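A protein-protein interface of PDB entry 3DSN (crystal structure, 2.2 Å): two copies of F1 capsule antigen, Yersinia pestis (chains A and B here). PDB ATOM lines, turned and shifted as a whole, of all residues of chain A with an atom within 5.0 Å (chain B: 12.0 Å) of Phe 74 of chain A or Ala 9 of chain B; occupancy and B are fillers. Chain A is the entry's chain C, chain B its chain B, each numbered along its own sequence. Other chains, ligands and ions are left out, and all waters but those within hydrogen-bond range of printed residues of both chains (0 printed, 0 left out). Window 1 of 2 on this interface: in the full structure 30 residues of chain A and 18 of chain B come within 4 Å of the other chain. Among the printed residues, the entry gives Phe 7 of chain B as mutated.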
ATOM      1  N   TYR A  23     -18.900 -11.355  16.824  1.00  0.00           N
ATOM      2  CA  TYR A  23     -17.625 -11.768  16.275  1.00  0.00           C
ATOM      3  C   TYR A  23     -16.467 -11.502  17.239  1.00  0.00           C
ATOM      4  O   TYR A  23     -16.433 -10.493  17.934  1.00  0.00           O
ATOM      5  CB  TYR A  23     -17.375 -11.031  14.962  1.00  0.00           C
ATOM      6  CG  TYR A  23     -16.075 -11.365  14.264  1.00  0.00           C
ATOM      7  CD1 TYR A  23     -15.940 -12.535  13.508  1.00  0.00           C
ATOM      8  CD2 TYR A  23     -14.978 -10.484  14.331  1.00  0.00           C
ATOM      9  CE1 TYR A  23     -14.709 -12.827  12.821  1.00  0.00           C
ATOM     10  CE2 TYR A  23     -13.790 -10.765  13.662  1.00  0.00           C
ATOM     11  CZ  TYR A  23     -13.663 -11.918  12.911  1.00  0.00           C
ATOM     12  OH  TYR A  23     -12.480 -12.157  12.281  1.00  0.00           O
ATOM     13  N   VAL A  43      -9.028 -17.034  11.901  1.00  0.00           N
ATOM     14  CA  VAL A  43      -9.082 -15.610  11.570  1.00  0.00           C
ATOM     15  C   VAL A  43      -9.940 -14.949  12.641  1.00  0.00           C
ATOM     16  O   VAL A  43      -9.612 -13.876  13.149  1.00  0.00           O
ATOM     17  CB  VAL A  43      -9.698 -15.381  10.150  1.00  0.00           C
ATOM     18  CG1 VAL A  43      -9.830 -13.875   9.805  1.00  0.00           C
ATOM     19  CG2 VAL A  43      -8.861 -16.141   9.049  1.00  0.00           C
ATOM     20  N   LEU A  72     -15.929 -16.766   2.384  1.00  0.00           N
ATOM     21  CA  LEU A  72     -16.006 -15.345   2.727  1.00  0.00           C
ATOM     22  C   LEU A  72     -14.719 -14.665   2.310  1.00  0.00           C
ATOM     23  O   LEU A  72     -13.631 -15.189   2.511  1.00  0.00           O
ATOM     24  CB  LEU A  72     -16.291 -15.112   4.213  1.00  0.00           C
ATOM     25  CG  LEU A  72     -17.635 -15.579   4.797  1.00  0.00           C
ATOM     26  CD1 LEU A  72     -17.608 -15.374   6.321  1.00  0.00           C
ATOM     27  CD2 LEU A  72     -18.860 -14.881   4.188  1.00  0.00           C
ATOM     28  N   THR A  73     -14.855 -13.488   1.718  1.00  0.00           N
ATOM     29  CA  THR A  73     -13.721 -12.726   1.208  1.00  0.00           C
ATOM     30  C   THR A  73     -13.508 -11.462   2.048  1.00  0.00           C
ATOM     31  O   THR A  73     -14.438 -10.717   2.263  1.00  0.00           O
ATOM     32  CB  THR A  73     -13.989 -12.354  -0.288  1.00  0.00           C
ATOM     33  OG1 THR A  73     -14.302 -13.554  -1.010  1.00  0.00           O
ATOM     34  CG2 THR A  73     -12.784 -11.703  -0.923  1.00  0.00           C
ATOM     35  N   PHE A  74     -12.282 -11.262   2.518  1.00  0.00           N
ATOM     36  CA  PHE A  74     -11.867 -10.105   3.290  1.00  0.00           C
ATOM     37  C   PHE A  74     -11.066  -9.204   2.381  1.00  0.00           C
ATOM     38  O   PHE A  74     -10.299  -9.686   1.567  1.00  0.00           O
ATOM     39  CB  PHE A  74     -10.954 -10.527   4.452  1.00  0.00           C
ATOM     40  CG  PHE A  74     -11.688 -11.162   5.604  1.00  0.00           C
ATOM     41  CD1 PHE A  74     -12.269 -12.421   5.463  1.00  0.00           C
ATOM     42  CD2 PHE A  74     -11.829 -10.482   6.814  1.00  0.00           C
ATOM     43  CE1 PHE A  74     -12.963 -13.003   6.523  1.00  0.00           C
ATOM     44  CE2 PHE A  74     -12.501 -11.043   7.867  1.00  0.00           C
ATOM     45  CZ  PHE A  74     -13.071 -12.314   7.742  1.00  0.00           C
ATOM     46  N   THR A  75     -11.213  -7.895   2.579  1.00  0.00           N
ATOM     47  CA  THR A  75     -10.591  -6.898   1.711  1.00  0.00           C
ATOM     48  C   THR A  75      -9.834  -5.896   2.560  1.00  0.00           C
ATOM     49  O   THR A  75     -10.271  -5.534   3.653  1.00  0.00           O
ATOM     50  CB  THR A  75     -11.668  -6.220   0.846  1.00  0.00           C
ATOM     51  OG1 THR A  75     -12.471  -7.248   0.265  1.00  0.00           O
ATOM     52  CG2 THR A  75     -11.064  -5.298  -0.264  1.00  0.00           C
ATOM     53  N   SER A  76      -8.670  -5.500   2.071  1.00  0.00           N
ATOM     54  CA  SER A  76      -7.876  -4.471   2.696  1.00  0.00           C
ATOM     55  C   SER A  76      -8.586  -3.128   2.732  1.00  0.00           C
ATOM     56  O   SER A  76      -9.460  -2.828   1.900  1.00  0.00           O
ATOM     57  CB  SER A  76      -6.529  -4.336   1.992  1.00  0.00           C
ATOM     58  OG  SER A  76      -6.688  -3.965   0.639  1.00  0.00           O
ATOM     59  N   HIS A  82      -6.602  -5.638  -1.844  1.00  0.00           N
ATOM     60  CA  HIS A  82      -5.970  -6.938  -1.556  1.00  0.00           C
ATOM     61  C   HIS A  82      -7.004  -7.821  -0.905  1.00  0.00           C
ATOM     62  O   HIS A  82      -7.741  -7.356  -0.024  1.00  0.00           O
ATOM     63  CB  HIS A  82      -4.777  -6.804  -0.596  1.00  0.00           C
ATOM     64  CG  HIS A  82      -3.684  -5.929  -1.108  1.00  0.00           C
ATOM     65  ND1 HIS A  82      -2.950  -6.242  -2.227  1.00  0.00           N
ATOM     66  CD2 HIS A  82      -3.196  -4.751  -0.653  1.00  0.00           C
ATOM     67  CE1 HIS A  82      -2.060  -5.294  -2.447  1.00  0.00           C
ATOM     68  NE2 HIS A  82      -2.184  -4.381  -1.501  1.00  0.00           N
ATOM     69  N   GLN A  83      -7.085  -9.080  -1.315  1.00  0.00           N
ATOM     70  CA  GLN A  83      -8.152  -9.952  -0.762  1.00  0.00           C
ATOM     71  C   GLN A  83      -7.652 -11.324  -0.330  1.00  0.00           C
ATOM     72  O   GLN A  83      -6.702 -11.845  -0.910  1.00  0.00           O
ATOM     73  CB  GLN A  83      -9.346 -10.078  -1.736  1.00  0.00           C
ATOM     74  CG  GLN A  83     -10.064  -8.709  -2.064  1.00  0.00           C
ATOM     75  CD  GLN A  83     -11.316  -8.910  -2.925  1.00  0.00           C
ATOM     76  OE1 GLN A  83     -11.265  -9.574  -3.970  1.00  0.00           O
ATOM     77  NE2 GLN A  83     -12.453  -8.349  -2.479  1.00  0.00           N
ATOM     78  N   PHE A  84      -8.284 -11.895   0.703  1.00  0.00           N
ATOM     79  CA  PHE A  84      -8.087 -13.309   0.993  1.00  0.00           C
ATOM     80  C   PHE A  84      -9.420 -13.986   1.304  1.00  0.00           C
ATOM     81  O   PHE A  84     -10.365 -13.347   1.759  1.00  0.00           O
ATOM     82  CB  PHE A  84      -7.038 -13.517   2.108  1.00  0.00           C
ATOM     83  CG  PHE A  84      -7.483 -13.043   3.475  1.00  0.00           C
ATOM     84  CD1 PHE A  84      -8.156 -13.902   4.341  1.00  0.00           C
ATOM     85  CD2 PHE A  84      -7.223 -11.747   3.899  1.00  0.00           C
ATOM     86  CE1 PHE A  84      -8.578 -13.482   5.609  1.00  0.00           C
ATOM     87  CE2 PHE A  84      -7.641 -11.316   5.173  1.00  0.00           C
ATOM     88  CZ  PHE A  84      -8.316 -12.189   6.023  1.00  0.00           C
ATOM     89  N   THR A  86     -11.754 -17.263   3.109  1.00  0.00           N
ATOM     90  CA  THR A  86     -11.894 -18.023   4.324  1.00  0.00           C
ATOM     91  C   THR A  86     -13.090 -18.933   4.166  1.00  0.00           C
ATOM     92  O   THR A  86     -14.008 -18.629   3.418  1.00  0.00           O
ATOM     93  CB  THR A  86     -12.201 -17.124   5.541  1.00  0.00           C
ATOM     94  OG1 THR A  86     -13.500 -16.557   5.390  1.00  0.00           O
ATOM     95  CG2 THR A  86     -11.169 -16.005   5.735  1.00  0.00           C
ATOM     96  N   VAL A 123     -13.959 -18.958  11.442  1.00  0.00           N
ATOM     97  CA  VAL A 123     -13.536 -18.401  10.176  1.00  0.00           C
ATOM     98  C   VAL A 123     -12.092 -18.848  10.001  1.00  0.00           C
ATOM     99  O   VAL A 123     -11.215 -18.432  10.740  1.00  0.00           O
ATOM    100  CB  VAL A 123     -13.664 -16.855  10.177  1.00  0.00           C
ATOM    101  CG1 VAL A 123     -13.198 -16.265   8.851  1.00  0.00           C
ATOM    102  CG2 VAL A 123     -15.112 -16.443  10.462  1.00  0.00           C
ATOM    103  N   TYR A 138      -8.215  -5.753   7.460  1.00  0.00           N
ATOM    104  CA  TYR A 138      -9.039  -6.405   6.451  1.00  0.00           C
ATOM    105  C   TYR A 138     -10.387  -6.538   7.105  1.00  0.00           C
ATOM    106  O   TYR A 138     -10.478  -6.735   8.326  1.00  0.00           O
ATOM    107  CB  TYR A 138      -8.461  -7.797   6.056  1.00  0.00           C
ATOM    108  CG  TYR A 138      -7.255  -7.702   5.125  1.00  0.00           C
ATOM    109  CD1 TYR A 138      -6.044  -7.139   5.559  1.00  0.00           C
ATOM    110  CD2 TYR A 138      -7.338  -8.138   3.789  1.00  0.00           C
ATOM    111  CE1 TYR A 138      -4.942  -7.008   4.686  1.00  0.00           C
ATOM    112  CE2 TYR A 138      -6.249  -8.044   2.923  1.00  0.00           C
ATOM    113  CZ  TYR A 138      -5.051  -7.473   3.388  1.00  0.00           C
ATOM    114  OH  TYR A 138      -4.005  -7.371   2.523  1.00  0.00           O
ATOM    115  N   THR A 139     -11.438  -6.416   6.305  1.00  0.00           N
ATOM    116  CA  THR A 139     -12.801  -6.551   6.798  1.00  0.00           C
ATOM    117  C   THR A 139     -13.684  -7.333   5.815  1.00  0.00           C
ATOM    118  O   THR A 139     -13.398  -7.418   4.617  1.00  0.00           O
ATOM    119  CB  THR A 139     -13.479  -5.168   7.054  1.00  0.00           C
ATOM    120  OG1 THR A 139     -13.732  -4.535   5.801  1.00  0.00           O
ATOM    121  CG2 THR A 139     -12.630  -4.264   7.901  1.00  0.00           C
ATOM    122  N   ASP A 140     -14.741  -7.919   6.343  1.00  0.00           N
ATOM    123  CA  ASP A 140     -15.818  -8.410   5.519  1.00  0.00           C
ATOM    124  C   ASP A 140     -17.142  -8.127   6.215  1.00  0.00           C
ATOM    125  O   ASP A 140     -17.354  -8.577   7.356  1.00  0.00           O
ATOM    126  CB  ASP A 140     -15.670  -9.914   5.287  1.00  0.00           C
ATOM    127  CG  ASP A 140     -16.543 -10.416   4.160  1.00  0.00           C
ATOM    128  OD1 ASP A 140     -16.977  -9.607   3.306  1.00  0.00           O
ATOM    129  OD2 ASP A 140     -16.788 -11.633   4.131  1.00  0.00           O
ATOM    130  N   ALA A 141     -18.027  -7.376   5.543  1.00  0.00           N
ATOM    131  CA  ALA A 141     -19.376  -7.184   6.045  1.00  0.00           C
ATOM    132  C   ALA A 141     -20.182  -8.436   5.729  1.00  0.00           C
ATOM    133  O   ALA A 141     -20.473  -8.743   4.552  1.00  0.00           O
ATOM    134  CB  ALA A 141     -20.033  -5.929   5.466  1.00  0.00           C
ATOM    135  N   VAL A 142     -20.527  -9.163   6.794  1.00  0.00           N
ATOM    136  CA  VAL A 142     -21.126 -10.480   6.664  1.00  0.00           C
ATOM    137  C   VAL A 142     -22.580 -10.335   7.064  1.00  0.00           C
ATOM    138  O   VAL A 142     -22.878  -9.745   8.079  1.00  0.00           O
ATOM    139  CB  VAL A 142     -20.377 -11.548   7.582  1.00  0.00           C
ATOM    140  CG1 VAL A 142     -21.092 -12.893   7.592  1.00  0.00           C
ATOM    141  CG2 VAL A 142     -18.939 -11.731   7.137  1.00  0.00           C
ATOM    142  N   ALA B   5     -29.219 -11.103  10.407  1.00  0.00           N
ATOM    143  CA  ALA B   5     -28.383 -10.216  11.188  1.00  0.00           C
ATOM    144  C   ALA B   5     -27.111  -9.964  10.371  1.00  0.00           C
ATOM    145  O   ALA B   5     -26.899 -10.568   9.330  1.00  0.00           O
ATOM    146  CB  ALA B   5     -28.060 -10.858  12.565  1.00  0.00           C
ATOM    147  N   SER B   6     -26.253  -9.086  10.848  1.00  0.00           N
ATOM    148  CA  SER B   6     -25.014  -8.787  10.138  1.00  0.00           C
ATOM    149  C   SER B   6     -23.929  -8.403  11.147  1.00  0.00           C
ATOM    150  O   SER B   6     -24.237  -7.997  12.253  1.00  0.00           O
ATOM    151  CB  SER B   6     -25.246  -7.643   9.127  1.00  0.00           C
ATOM    152  OG  SER B   6     -25.608  -6.474   9.841  1.00  0.00           O
ATOM    153  N   PHE B   7     -22.667  -8.550  10.761  1.00  0.00           N
ATOM    154  CA  PHE B   7     -21.542  -8.000  11.543  1.00  0.00           C
ATOM    155  C   PHE B   7     -20.392  -7.830  10.584  1.00  0.00           C
ATOM    156  O   PHE B   7     -20.262  -8.611   9.648  1.00  0.00           O
ATOM    157  CB  PHE B   7     -21.071  -8.970  12.637  1.00  0.00           C
ATOM    158  CG  PHE B   7     -20.340  -8.283  13.759  1.00  0.00           C
ATOM    159  CD1 PHE B   7     -21.051  -7.645  14.772  1.00  0.00           C
ATOM    160  CD2 PHE B   7     -18.950  -8.232  13.786  1.00  0.00           C
ATOM    161  CE1 PHE B   7     -20.392  -6.998  15.812  1.00  0.00           C
ATOM    162  CE2 PHE B   7     -18.281  -7.560  14.837  1.00  0.00           C
ATOM    163  CZ  PHE B   7     -19.012  -6.959  15.840  1.00  0.00           C
ATOM    164  N   THR B   8     -19.535  -6.841  10.830  1.00  0.00           N
ATOM    165  CA  THR B   8     -18.324  -6.729  10.030  1.00  0.00           C
ATOM    166  C   THR B   8     -17.171  -7.508  10.673  1.00  0.00           C
ATOM    167  O   THR B   8     -16.613  -7.092  11.667  1.00  0.00           O
ATOM    168  CB  THR B   8     -17.936  -5.261   9.796  1.00  0.00           C
ATOM    169  OG1 THR B   8     -19.003  -4.606   9.128  1.00  0.00           O
ATOM    170  CG2 THR B   8     -16.682  -5.144   8.909  1.00  0.00           C
ATOM    171  N   ALA B   9     -16.849  -8.646  10.089  1.00  0.00           N
ATOM    172  CA  ALA B   9     -15.680  -9.421  10.446  1.00  0.00           C
ATOM    173  C   ALA B   9     -14.414  -8.623  10.137  1.00  0.00           C
ATOM    174  O   ALA B   9     -14.373  -7.892   9.163  1.00  0.00           O
ATOM    175  CB  ALA B   9     -15.708 -10.766   9.683  1.00  0.00           C
ATOM    176  N   THR B  10     -13.421  -8.735  11.017  1.00  0.00           N
ATOM    177  CA  THR B  10     -12.161  -7.990  10.928  1.00  0.00           C
ATOM    178  C   THR B  10     -10.961  -8.922  11.012  1.00  0.00           C
ATOM    179  O   THR B  10     -11.047  -9.962  11.649  1.00  0.00           O
ATOM    180  CB  THR B  10     -12.043  -6.963  12.076  1.00  0.00           C
ATOM    181  OG1 THR B  10     -12.165  -7.632  13.345  1.00  0.00           O
ATOM    182  CG2 THR B  10     -13.167  -5.871  11.979  1.00  0.00           C
ATOM    183  N   ALA B  11      -9.864  -8.578  10.342  1.00  0.00           N
ATOM    184  CA  ALA B  11      -8.623  -9.325  10.467  1.00  0.00           C
ATOM    185  C   ALA B  11      -7.465  -8.357  10.383  1.00  0.00           C
ATOM    186  O   ALA B  11      -7.556  -7.313   9.752  1.00  0.00           O
ATOM    187  CB  ALA B  11      -8.496 -10.433   9.403  1.00  0.00           C
ATOM    188  N   THR B  12      -6.375  -8.699  11.054  1.00  0.00           N
ATOM    189  CA  THR B  12      -5.155  -7.899  11.025  1.00  0.00           C
ATOM    190  C   THR B  12      -4.067  -8.755  10.424  1.00  0.00           C
ATOM    191  O   THR B  12      -3.845  -9.855  10.901  1.00  0.00           O
ATOM    192  CB  THR B  12      -4.798  -7.416  12.443  1.00  0.00           C
ATOM    193  OG1 THR B  12      -5.901  -6.674  12.948  1.00  0.00           O
ATOM    194  CG2 THR B  12      -3.603  -6.480  12.457  1.00  0.00           C
ATOM    195  N   LEU B  13      -3.461  -8.290   9.332  1.00  0.00           N
ATOM    196  CA  LEU B  13      -2.363  -9.007   8.692  1.00  0.00           C
ATOM    197  C   LEU B  13      -1.077  -8.207   8.894  1.00  0.00           C
ATOM    198  O   LEU B  13      -1.081  -6.998   8.850  1.00  0.00           O
ATOM    199  CB  LEU B  13      -2.598  -9.270   7.198  1.00  0.00           C
ATOM    200  CG  LEU B  13      -3.871  -9.741   6.477  1.00  0.00           C
ATOM    201  CD1 LEU B  13      -3.507 -10.479   5.186  1.00  0.00           C
ATOM    202  CD2 LEU B  13      -4.950 -10.495   7.326  1.00  0.00           C
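Printed residues of chain B within 4 Å of Phe 74 of chain A: Ala 9 (3.6 Å).
Val 43 of chain A touches just one residue of chain B: Ala 11.
No residue of chain B comes within 4 Å of Leu 72 of chain A.
No residue of chain B comes within 4 Å of Thr 73 of chain A.
No residue of chain B comes within 4 Å of Gln 83 of chain A.
No residue of chain B comes within 4 Å of Thr 86 of chain A.
No residue of chain B comes within 4 Å of Val 123 of chain A.
Tyr 138 of chain A touches just these residues of chain B: Thr 10 (3.3 Å), Ala 11 (2.8 Å) and Leu 13 (3.4 Å).
Thr 139 of chain A touches just these residues of chain B: Thr 8 and Ala 9.
Of chain B, only Phe 7 (3.9 Å) comes within 4 Å of Ala 141 of chain A.
Val 142 of chain A touches just these residues of chain B: Ser 6 (3.1 Å) and Phe 7 (2.9 Å).
Of the printed residues of chain A, Ala 11 of chain B touches Val 43 (3.7 Å), Phe 84 (3.8 Å) and Tyr 138 (2.8 Å).
Of the printed residues of chain A, Phe 7 of chain B touches Tyr 23 (3.4 Å), Asp 140 (3.7 Å), Ala 141 (3.9 Å) and Val 142 (2.9 Å).
Printed residues of chain A within 4 Å of Ser 6 of chain B: Val 142 (3.1 Å).
His 82 of chain A touches none of the printed residues of chain B.
Thr 12 of chain B touches none of the printed residues of chain A.
N of Val 43 of chain A sits at hydrogen-bond distance from O of Val 123 of chain A (2.8 Å).
The backbone NH (N) of Phe 74 of chain A lies within hydrogen-bond range of the backbone carbonyl oxygen (O) of Phe 84 of chain A (2.9 Å).
The backbone carbonyl oxygen of Val 43 of chain A is in hydrogen-bond range of the side-chain hydroxyl of Tyr 23 of chain A (3.5 Å).
The backbone NH (N) of Thr 75 of chain A lies within hydrogen-bond range of the backbone carbonyl oxygen (O) of Thr 139 of chain A, at 3.0 Å.
Tyr 23 of chain A touches Phe 7 of chain B.
CZ of Phe 84 of chain A touches CB of Ala 11 of chain B (3.8 Å).
CD2 of Leu 13 of chain B touches CE2 of Phe 84 of chain A, 3.5 Å away.
Thr 10 of chain B touches Tyr 138 of chain A (CA to O, 3.3 Å).
CE1 of Tyr 138 of chain A touches CG of Leu 13 of chain B, 3.4 Å away.
CG2 of Thr 8 of chain B touches CB of Thr 139 of chain A, 3.7 Å away.
Asp 140 of chain A touches Phe 7 of chain B (O to O, 3.7 Å).
Asp 140 of chain A touches Thr 8 of chain B.
C of Ala 141 of chain A touches O of Phe 7 of chain B (3.9 Å).
CA of Ser 6 of chain B touches O of Val 142 of chain A (3.1 Å).
No position is printed for both chains.
Of the 18 pairs that touch across the chains among the printed residues, none has its exchanged pair printed and touching as well.
The side-chain hydroxyl of Tyr 23 of chain A lies within hydrogen-bond range of the backbone carbonyl oxygen of Thr 10 of chain B (2.7 Å).
The backbone NH (N) of Ala 9 of chain B sits at hydrogen-bond distance from the backbone carbonyl oxygen (O) of Asp 140 of chain A (2.8 Å).
N of Ala 11 of chain B is in hydrogen-bond range of O of Tyr 138 of chain A (2.8 Å).
The backbone carbonyl oxygen (O) of Phe 7 of chain B lies within hydrogen-bond range of the backbone NH (N) of Val 142 of chain A, 2.9 Å away.
Printed residues of chain B that touch a printed residue of chain A: Ser 6, Phe 7, Thr 8, Ala 9, Thr 10, Ala 11 and Leu 13.
Hydrophobic or aromatic side chains of chain B within 4 Å of the printed part of chain A: Phe 7, Ala 9, Ala 11 and Leu 13.
Among the printed residues, no Asp or Glu carboxylate lies within 4 Å of a Lys or Arg side-chain nitrogen of the other chain.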
